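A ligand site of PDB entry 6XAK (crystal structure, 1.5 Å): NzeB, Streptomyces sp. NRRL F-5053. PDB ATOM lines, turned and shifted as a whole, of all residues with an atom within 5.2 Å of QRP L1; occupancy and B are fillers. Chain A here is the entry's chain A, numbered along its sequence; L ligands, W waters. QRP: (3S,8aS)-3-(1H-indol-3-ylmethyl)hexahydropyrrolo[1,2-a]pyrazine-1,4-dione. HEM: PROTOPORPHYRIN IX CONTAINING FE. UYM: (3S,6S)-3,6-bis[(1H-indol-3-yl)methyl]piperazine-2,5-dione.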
ATOM      1  N   GLN A  75      -0.901  -9.260  37.080  1.00  0.00           N
ATOM      2  CA  GLN A  75      -2.337  -9.314  37.298  1.00  0.00           C
ATOM      3  C   GLN A  75      -2.863 -10.748  37.384  1.00  0.00           C
ATOM      4  O   GLN A  75      -3.891 -10.998  38.018  1.00  0.00           O
ATOM      5  CB  GLN A  75      -3.063  -8.558  36.171  1.00  0.00           C
ATOM      6  CG  GLN A  75      -2.924  -9.220  34.807  1.00  0.00           C
ATOM      7  CD  GLN A  75      -3.129  -8.237  33.665  1.00  0.00           C
ATOM      8  OE1 GLN A  75      -4.260  -7.868  33.351  1.00  0.00           O
ATOM      9  NE2 GLN A  75      -2.041  -7.835  33.013  1.00  0.00           N
ATOM     10  N   GLU A  76      -2.203 -11.708  36.697  1.00  0.00           N
ATOM     11  CA  GLU A  76      -2.751 -13.055  36.604  1.00  0.00           C
ATOM     12  C   GLU A  76      -2.460 -13.846  37.890  1.00  0.00           C
ATOM     13  O   GLU A  76      -1.392 -13.669  38.501  1.00  0.00           O
ATOM     14  CB  GLU A  76      -2.188 -13.802  35.388  1.00  0.00           C
ATOM     15  CG  GLU A  76      -0.673 -13.989  35.345  1.00  0.00           C
ATOM     16  CD  GLU A  76       0.074 -12.855  34.657  1.00  0.00           C
ATOM     17  OE1 GLU A  76      -0.442 -11.710  34.603  1.00  0.00           O
ATOM     18  OE2 GLU A  76       1.217 -13.100  34.180  1.00  0.00           O
ATOM     19  N   LEU A  80       1.635 -17.938  33.650  1.00  0.00           N
ATOM     20  CA  LEU A  80       1.079 -18.490  32.415  1.00  0.00           C
ATOM     21  C   LEU A  80       2.096 -19.396  31.720  1.00  0.00           C
ATOM     22  O   LEU A  80       2.527 -19.164  30.605  1.00  0.00           O
ATOM     23  CB  LEU A  80       0.619 -17.365  31.503  1.00  0.00           C
ATOM     24  CG  LEU A  80      -0.323 -16.380  32.190  1.00  0.00           C
ATOM     25  CD1 LEU A  80      -0.763 -15.307  31.177  1.00  0.00           C
ATOM     26  CD2 LEU A  80      -1.498 -17.115  32.798  1.00  0.00           C
ATOM     27  N   PHE A 177      -8.987 -15.080  35.647  1.00  0.00           N
ATOM     28  CA  PHE A 177      -8.682 -14.360  36.872  1.00  0.00           C
ATOM     29  C   PHE A 177      -9.291 -15.024  38.108  1.00  0.00           C
ATOM     30  O   PHE A 177      -8.836 -14.786  39.221  1.00  0.00           O
ATOM     31  CB  PHE A 177      -9.187 -12.923  36.788  1.00  0.00           C
ATOM     32  CG  PHE A 177      -8.340 -12.027  35.935  1.00  0.00           C
ATOM     33  CD1 PHE A 177      -7.069 -11.629  36.361  1.00  0.00           C
ATOM     34  CD2 PHE A 177      -8.822 -11.545  34.704  1.00  0.00           C
ATOM     35  CE1 PHE A 177      -6.288 -10.809  35.583  1.00  0.00           C
ATOM     36  CE2 PHE A 177      -8.049 -10.716  33.919  1.00  0.00           C
ATOM     37  CZ  PHE A 177      -6.776 -10.335  34.348  1.00  0.00           C
ATOM     38  N   THR A 244      -8.802 -15.731  21.960  1.00  0.00           N
ATOM     39  CA  THR A 244      -8.940 -14.427  21.340  1.00  0.00           C
ATOM     40  C   THR A 244      -9.903 -14.485  20.168  1.00  0.00           C
ATOM     41  O   THR A 244     -10.855 -13.700  20.091  1.00  0.00           O
ATOM     42  CB  THR A 244      -7.562 -13.986  20.861  1.00  0.00           C
ATOM     43  OG1 THR A 244      -6.989 -15.060  20.099  1.00  0.00           O
ATOM     44  CG2 THR A 244      -6.638 -13.695  22.042  1.00  0.00           C
ATOM     45  N   LEU A 286     -12.661  -7.063  24.515  1.00  0.00           N
ATOM     46  CA  LEU A 286     -12.189  -8.432  24.510  1.00  0.00           C
ATOM     47  C   LEU A 286     -11.558  -8.798  25.850  1.00  0.00           C
ATOM     48  O   LEU A 286     -12.197  -9.438  26.700  1.00  0.00           O
ATOM     49  CB  LEU A 286     -11.225  -8.686  23.357  1.00  0.00           C
ATOM     50  CG  LEU A 286     -10.772 -10.146  23.166  1.00  0.00           C
ATOM     51  CD1 LEU A 286     -11.948 -11.148  22.990  1.00  0.00           C
ATOM     52  CD2 LEU A 286      -9.803 -10.218  21.998  1.00  0.00           C
ATOM     53  N   SER A 287     -10.317  -8.361  26.095  1.00  0.00           N
ATOM     54  CA  SER A 287      -9.671  -8.700  27.349  1.00  0.00           C
ATOM     55  C   SER A 287     -10.354  -8.009  28.539  1.00  0.00           C
ATOM     56  O   SER A 287     -10.744  -6.834  28.465  1.00  0.00           O
ATOM     57  CB  SER A 287      -8.184  -8.346  27.281  1.00  0.00           C
ATOM     58  OG  SER A 287      -7.515  -8.676  28.505  1.00  0.00           O
ATOM     59  N   THR A 288     -10.460  -8.739  29.655  1.00  0.00           N
ATOM     60  CA  THR A 288     -10.852  -8.181  30.949  1.00  0.00           C
ATOM     61  C   THR A 288      -9.633  -7.745  31.768  1.00  0.00           C
ATOM     62  O   THR A 288      -9.791  -7.264  32.904  1.00  0.00           O
ATOM     63  CB  THR A 288     -11.640  -9.223  31.746  1.00  0.00           C
ATOM     64  OG1 THR A 288     -10.820 -10.376  31.994  1.00  0.00           O
ATOM     65  CG2 THR A 288     -12.910  -9.635  30.994  1.00  0.00           C
ATOM     66  N   GLY A 289      -8.431  -7.933  31.240  1.00  0.00           N
ATOM     67  CA  GLY A 289      -7.223  -7.427  31.870  1.00  0.00           C
ATOM     68  C   GLY A 289      -6.569  -6.368  31.004  1.00  0.00           C
ATOM     69  O   GLY A 289      -7.250  -5.646  30.258  1.00  0.00           O
ATOM     70  N   SER A 290      -5.240  -6.245  31.094  1.00  0.00           N
ATOM     71  CA  SER A 290      -4.511  -5.195  30.411  1.00  0.00           C
ATOM     72  C   SER A 290      -3.244  -5.752  29.767  1.00  0.00           C
ATOM     73  O   SER A 290      -2.631  -6.705  30.274  1.00  0.00           O
ATOM     74  CB  SER A 290      -4.141  -4.116  31.428  1.00  0.00           C
ATOM     75  OG  SER A 290      -5.271  -3.322  31.762  1.00  0.00           O
ATOM     76  N   VAL A 291      -2.848  -5.146  28.648  1.00  0.00           N
ATOM     77  CA  VAL A 291      -1.474  -5.317  28.195  1.00  0.00           C
ATOM     78  C   VAL A 291      -0.575  -4.695  29.264  1.00  0.00           C
ATOM     79  O   VAL A 291      -0.998  -3.822  30.020  1.00  0.00           O
ATOM     80  CB  VAL A 291      -1.211  -4.676  26.816  1.00  0.00           C
ATOM     81  CG1 VAL A 291      -2.177  -5.242  25.773  1.00  0.00           C
ATOM     82  CG2 VAL A 291      -1.296  -3.187  26.888  1.00  0.00           C
ATOM     83  N   LYS A 292       0.658  -5.181  29.358  1.00  0.00           N
ATOM     84  CA  LYS A 292       1.503  -4.682  30.437  1.00  0.00           C
ATOM     85  C   LYS A 292       2.972  -4.736  30.037  1.00  0.00           C
ATOM     86  O   LYS A 292       3.385  -5.561  29.226  1.00  0.00           O
ATOM     87  CB  LYS A 292       1.222  -5.432  31.754  1.00  0.00           C
ATOM     88  CG  LYS A 292       1.889  -6.801  31.936  1.00  0.00           C
ATOM     89  CD  LYS A 292       1.464  -7.813  30.874  1.00  0.00           C
ATOM     90  CE  LYS A 292       1.885  -9.214  31.294  1.00  0.00           C
ATOM     91  NZ  LYS A 292       1.601 -10.133  30.164  1.00  0.00           N
ATOM     92  N   LEU A 316      -6.810  -1.866  27.026  1.00  0.00           N
ATOM     93  CA  LEU A 316      -7.119  -1.485  25.649  1.00  0.00           C
ATOM     94  C   LEU A 316      -8.565  -1.042  25.524  1.00  0.00           C
ATOM     95  O   LEU A 316      -8.873  -0.140  24.707  1.00  0.00           O
ATOM     96  CB  LEU A 316      -6.850  -2.675  24.724  1.00  0.00           C
ATOM     97  CG  LEU A 316      -5.432  -3.244  24.791  1.00  0.00           C
ATOM     98  CD1 LEU A 316      -5.361  -4.406  23.769  1.00  0.00           C
ATOM     99  CD2 LEU A 316      -4.392  -2.184  24.488  1.00  0.00           C
ATOM    100  N   GLY A 343      -7.286  -2.102  19.481  1.00  0.00           N
ATOM    101  CA  GLY A 343      -7.772  -3.476  19.606  1.00  0.00           C
ATOM    102  C   GLY A 343      -6.694  -4.527  19.384  1.00  0.00           C
ATOM    103  O   GLY A 343      -6.810  -5.637  19.884  1.00  0.00           O
ATOM    104  N   PHE A 390      -9.823 -14.224  30.909  1.00  0.00           N
ATOM    105  CA  PHE A 390      -9.050 -13.087  30.377  1.00  0.00           C
ATOM    106  C   PHE A 390      -9.720 -12.525  29.128  1.00  0.00           C
ATOM    107  O   PHE A 390      -9.677 -11.310  28.885  1.00  0.00           O
ATOM    108  CB  PHE A 390      -7.658 -13.554  29.940  1.00  0.00           C
ATOM    109  CG  PHE A 390      -6.745 -13.951  31.057  1.00  0.00           C
ATOM    110  CD1 PHE A 390      -7.079 -13.729  32.382  1.00  0.00           C
ATOM    111  CD2 PHE A 390      -5.518 -14.529  30.767  1.00  0.00           C
ATOM    112  CE1 PHE A 390      -6.205 -14.111  33.417  1.00  0.00           C
ATOM    113  CE2 PHE A 390      -4.657 -14.921  31.786  1.00  0.00           C
ATOM    114  CZ  PHE A 390      -4.991 -14.699  33.112  1.00  0.00           C
ATOM    115  N   PHE A 391     -10.287 -13.388  28.288  1.00  0.00           N
ATOM    116  CA  PHE A 391     -10.846 -12.996  27.004  1.00  0.00           C
ATOM    117  C   PHE A 391     -12.341 -13.320  27.020  1.00  0.00           C
ATOM    118  O   PHE A 391     -12.728 -14.498  26.960  1.00  0.00           O
ATOM    119  CB  PHE A 391     -10.092 -13.667  25.879  1.00  0.00           C
ATOM    120  CG  PHE A 391      -8.609 -13.387  25.920  1.00  0.00           C
ATOM    121  CD1 PHE A 391      -8.142 -12.120  25.646  1.00  0.00           C
ATOM    122  CD2 PHE A 391      -7.691 -14.375  26.289  1.00  0.00           C
ATOM    123  CE1 PHE A 391      -6.782 -11.837  25.688  1.00  0.00           C
ATOM    124  CE2 PHE A 391      -6.330 -14.092  26.331  1.00  0.00           C
ATOM    125  CZ  PHE A 391      -5.871 -12.811  26.042  1.00  0.00           C
HETATM  126  C   QRP L   1      -2.118 -10.085  28.943  1.00  0.00           C
HETATM  127  N   QRP L   1      -4.496  -9.838  28.363  1.00  0.00           N
HETATM  128  O   QRP L   1      -0.988  -9.657  28.810  1.00  0.00           O
HETATM  129  CA  QRP L   1      -3.135  -9.891  27.854  1.00  0.00           C
HETATM  130  CB  QRP L   1      -2.846  -8.633  27.025  1.00  0.00           C
HETATM  131  CG  QRP L   1      -4.027  -8.405  26.095  1.00  0.00           C
HETATM  132  OAA QRP L   1      -6.100 -10.548  29.821  1.00  0.00           O
HETATM  133  CAH QRP L   1      -2.638 -11.740  32.166  1.00  0.00           C
HETATM  134  CAI QRP L   1      -4.006 -11.254  31.719  1.00  0.00           C
HETATM  135  CAJ QRP L   1      -1.650 -11.093  31.187  1.00  0.00           C
HETATM  136  CAN QRP L   1      -4.929 -10.521  29.447  1.00  0.00           C
HETATM  137  CAT QRP L   1      -3.852 -11.268  30.203  1.00  0.00           C
HETATM  138  NAU QRP L   1      -2.493 -10.773  30.024  1.00  0.00           N
HETATM  139  CD1 QRP L   1      -4.953  -7.390  26.245  1.00  0.00           C
HETATM  140  CD2 QRP L   1      -4.422  -9.141  24.973  1.00  0.00           C
HETATM  141  NE1 QRP L   1      -5.875  -7.464  25.242  1.00  0.00           N
HETATM  142  CE2 QRP L   1      -5.577  -8.519  24.479  1.00  0.00           C
HETATM  143  CE3 QRP L   1      -3.888 -10.263  24.355  1.00  0.00           C
HETATM  144  CH2 QRP L   1      -5.683 -10.148  22.734  1.00  0.00           C
HETATM  145  CZ2 QRP L   1      -6.217  -9.025  23.352  1.00  0.00           C
HETATM  146  CZ3 QRP L   1      -4.514 -10.764  23.220  1.00  0.00           C
HETATM  147  CHA HEM L   2      -0.543 -10.117  20.510  1.00  0.00           C
HETATM  148  CHB HEM L   2      -5.207  -8.914  19.878  1.00  0.00           C
HETATM  149  CHC HEM L   2      -5.905 -12.940  17.245  1.00  0.00           C
HETATM  150  CHD HEM L   2      -1.184 -14.056  17.797  1.00  0.00           C
HETATM  151  C1A HEM L   2      -1.740  -9.431  20.542  1.00  0.00           C
HETATM  152  C2A HEM L   2      -1.967  -8.171  21.212  1.00  0.00           C
HETATM  153  C3A HEM L   2      -3.244  -7.846  21.043  1.00  0.00           C
HETATM  154  C4A HEM L   2      -3.890  -8.891  20.263  1.00  0.00           C
HETATM  155  CMA HEM L   2      -3.909  -6.574  21.598  1.00  0.00           C
HETATM  156  CAA HEM L   2      -0.940  -7.282  21.954  1.00  0.00           C
HETATM  157  CBA HEM L   2      -0.544  -7.780  23.343  1.00  0.00           C
HETATM  158  CGA HEM L   2       0.463  -6.858  23.989  1.00  0.00           C
HETATM  159  O1A HEM L   2       0.687  -5.712  23.516  1.00  0.00           O
HETATM  160  O2A HEM L   2       1.077  -7.269  25.011  1.00  0.00           O
HETATM  161  C1B HEM L   2      -5.797  -9.902  19.113  1.00  0.00           C
HETATM  162  C2B HEM L   2      -7.194  -9.900  18.696  1.00  0.00           C
HETATM  163  C3B HEM L   2      -7.388 -11.042  17.980  1.00  0.00           C
HETATM  164  C4B HEM L   2      -6.116 -11.745  17.908  1.00  0.00           C
HETATM  165  CMB HEM L   2      -8.186  -8.785  19.101  1.00  0.00           C
HETATM  166  CAB HEM L   2      -8.677 -11.547  17.284  1.00  0.00           C
HETATM  167  CBB HEM L   2      -9.721 -10.746  17.038  1.00  0.00           C
HETATM  168  C1C HEM L   2      -4.675 -13.590  17.165  1.00  0.00           C
HETATM  169  C2C HEM L   2      -4.428 -14.820  16.453  1.00  0.00           C
HETATM  170  C3C HEM L   2      -3.150 -15.144  16.622  1.00  0.00           C
HETATM  171  C4C HEM L   2      -2.510 -14.119  17.426  1.00  0.00           C
HETATM  172  CMC HEM L   2      -5.503 -15.598  15.675  1.00  0.00           C
HETATM  173  CAC HEM L   2      -2.497 -16.406  16.005  1.00  0.00           C
HETATM  174  CBC HEM L   2      -1.583 -17.123  16.654  1.00  0.00           C
HETATM  175  C1D HEM L   2      -0.617 -13.148  18.657  1.00  0.00           C
HETATM  176  C2D HEM L   2       0.688 -13.257  19.289  1.00  0.00           C
HETATM  177  C3D HEM L   2       0.864 -12.170  20.067  1.00  0.00           C
HETATM  178  C4D HEM L   2      -0.319 -11.344  19.921  1.00  0.00           C
HETATM  179  CMD HEM L   2       1.673 -14.438  19.128  1.00  0.00           C
HETATM  180  CAD HEM L   2       2.074 -11.811  20.982  1.00  0.00           C
HETATM  181  CBD HEM L   2       3.046 -10.870  20.315  1.00  0.00           C
HETATM  182  CGD HEM L   2       4.034 -10.282  21.303  1.00  0.00           C
HETATM  183  O1D HEM L   2       3.892 -10.437  22.542  1.00  0.00           O
HETATM  184  O2D HEM L   2       5.007  -9.648  20.824  1.00  0.00           O
HETATM  185  NA  HEM L   2      -2.928  -9.845  19.976  1.00  0.00           N
HETATM  186  NB  HEM L   2      -5.161 -11.046  18.628  1.00  0.00           N
HETATM  187  NC  HEM L   2      -3.473 -13.174  17.731  1.00  0.00           N
HETATM  188  ND  HEM L   2      -1.197 -11.958  19.064  1.00  0.00           N
HETATM  189 FE   HEM L   2      -3.146 -11.360  18.625  1.00  0.00          FE
HETATM  190  N   UYM L   3       1.518 -17.672  28.298  1.00  0.00           N
HETATM  191  C   UYM L   3       3.053 -13.591  24.499  1.00  0.00           C
HETATM  192  O   UYM L   3       3.415 -14.030  23.448  1.00  0.00           O
HETATM  193  C1  UYM L   3       2.944 -14.550  25.698  1.00  0.00           C
HETATM  194  C10 UYM L   3       2.635 -20.017  27.753  1.00  0.00           C
HETATM  195  C11 UYM L   3       2.288 -11.515  25.834  1.00  0.00           C
HETATM  196  C12 UYM L   3       0.841 -10.961  25.705  1.00  0.00           C
HETATM  197  C15 UYM L   3       2.311 -12.449  27.044  1.00  0.00           C
HETATM  198  C2  UYM L   3       1.885 -15.623  25.411  1.00  0.00           C
HETATM  199  C3  UYM L   3       1.877 -16.754  26.508  1.00  0.00           C
HETATM  200  C34 UYM L   3      -0.238 -11.992  25.185  1.00  0.00           C
HETATM  201  C35 UYM L   3      -0.414 -12.067  23.938  1.00  0.00           C
HETATM  202  C37 UYM L   3      -1.775 -13.487  25.111  1.00  0.00           C
HETATM  203  C38 UYM L   3      -0.949 -12.731  25.934  1.00  0.00           C
HETATM  204  C39 UYM L   3      -1.036 -12.897  27.334  1.00  0.00           C
HETATM  205  C4  UYM L   3       1.331 -16.530  27.669  1.00  0.00           C
HETATM  206  C40 UYM L   3      -1.935 -13.840  27.878  1.00  0.00           C
HETATM  207  C41 UYM L   3      -2.761 -14.587  27.037  1.00  0.00           C
HETATM  208  C42 UYM L   3      -2.691 -14.420  25.661  1.00  0.00           C
HETATM  209  C5  UYM L   3       2.196 -18.701  27.579  1.00  0.00           C
HETATM  210  C6  UYM L   3       2.429 -18.002  26.338  1.00  0.00           C
HETATM  211  C7  UYM L   3       3.107 -18.691  25.326  1.00  0.00           C
HETATM  212  C8  UYM L   3       3.555 -20.012  25.497  1.00  0.00           C
HETATM  213  C9  UYM L   3       3.320 -20.685  26.717  1.00  0.00           C
HETATM  214  N1  UYM L   3       2.623 -13.854  26.923  1.00  0.00           N
HETATM  215  N2  UYM L   3       2.739 -12.178  24.635  1.00  0.00           N
HETATM  216  N36 UYM L   3      -1.412 -13.048  23.728  1.00  0.00           N
HETATM  217  O1  UYM L   3       2.075 -11.997  28.113  1.00  0.00           O
HETATM  218  O   HOH W   1       0.721  -7.710  27.660  1.00  0.00           O
HETATM  219  O   HOH W   2      -8.460  -6.518  24.524  1.00  0.00           O
HETATM  220  O   HOH W   3      -2.975 -13.116  21.207  1.00  0.00           O
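The side-chain hydroxyl (OG) of Ser 287 is in hydrogen-bond range of an oxygen (OAA) of QRP L1, at 2.7 Å. NZ of Lys 292 is in hydrogen-bond range of O1 of UYM L3, 2.8 Å away. O of Leu 80 is in hydrogen-bond range of N of UYM L3 (2.9 Å). NZ of Lys 292 is in hydrogen-bond range of O of QRP L1, 3.0 Å away.
An oxygen (O1D) of HEM L2 lies within hydrogen-bond range of a nitrogen (N2) of UYM L3 (3.0 Å).
The backbone carbonyl oxygen (O) of Phe 390 sits close to the side-chain hydroxyl (OG) of Ser 287 (3.4 Å). The backbone NH of Gly 289 sits at hydrogen-bond distance from the side-chain hydroxyl of Ser 287 (3.0 Å). N of Thr 288 lies within hydrogen-bond range of O of Phe 390, 2.8 Å away. The side-chain amide oxygen (OE1) of Gln 75 is in hydrogen-bond range of the backbone NH (N) of Ser 290.
Gln 75 touches QRP L1. OE1 of Glu 76 touches CAH of QRP L1, at 3.3 Å. Phe 177 touches QRP L1. Thr 244 touches QRP L1 (CG2 to CH2, 3.7 Å). N of Gly 289 touches OAA of QRP L1, 3.8 Å away. Ser 290 touches QRP L1. Val 291 touches QRP L1 (CG1 to CD1, 3.5 Å). Leu 316 touches QRP L1. Phe 390 touches QRP L1. Phe 391 touches QRP L1 (CE1 to CZ3, 3.5 Å). Hydrophobic or aromatic side chains within 4 Å of QRP L1: Phe 177, Val 291, Leu 316, Phe 390 and Phe 391. Along chain A the residues within 4 Å of QRP L1 span positions 75 to 391.
Water W1 lies within hydrogen-bond range of O2A of HEM L2 (2.7 Å), O of QRP L1 (2.8 Å) and N of Lys 292 (3.0 Å). Water W2 bridges NE1 of QRP L1 (2.8 Å) and N of Ser 287 (3.1 Å).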
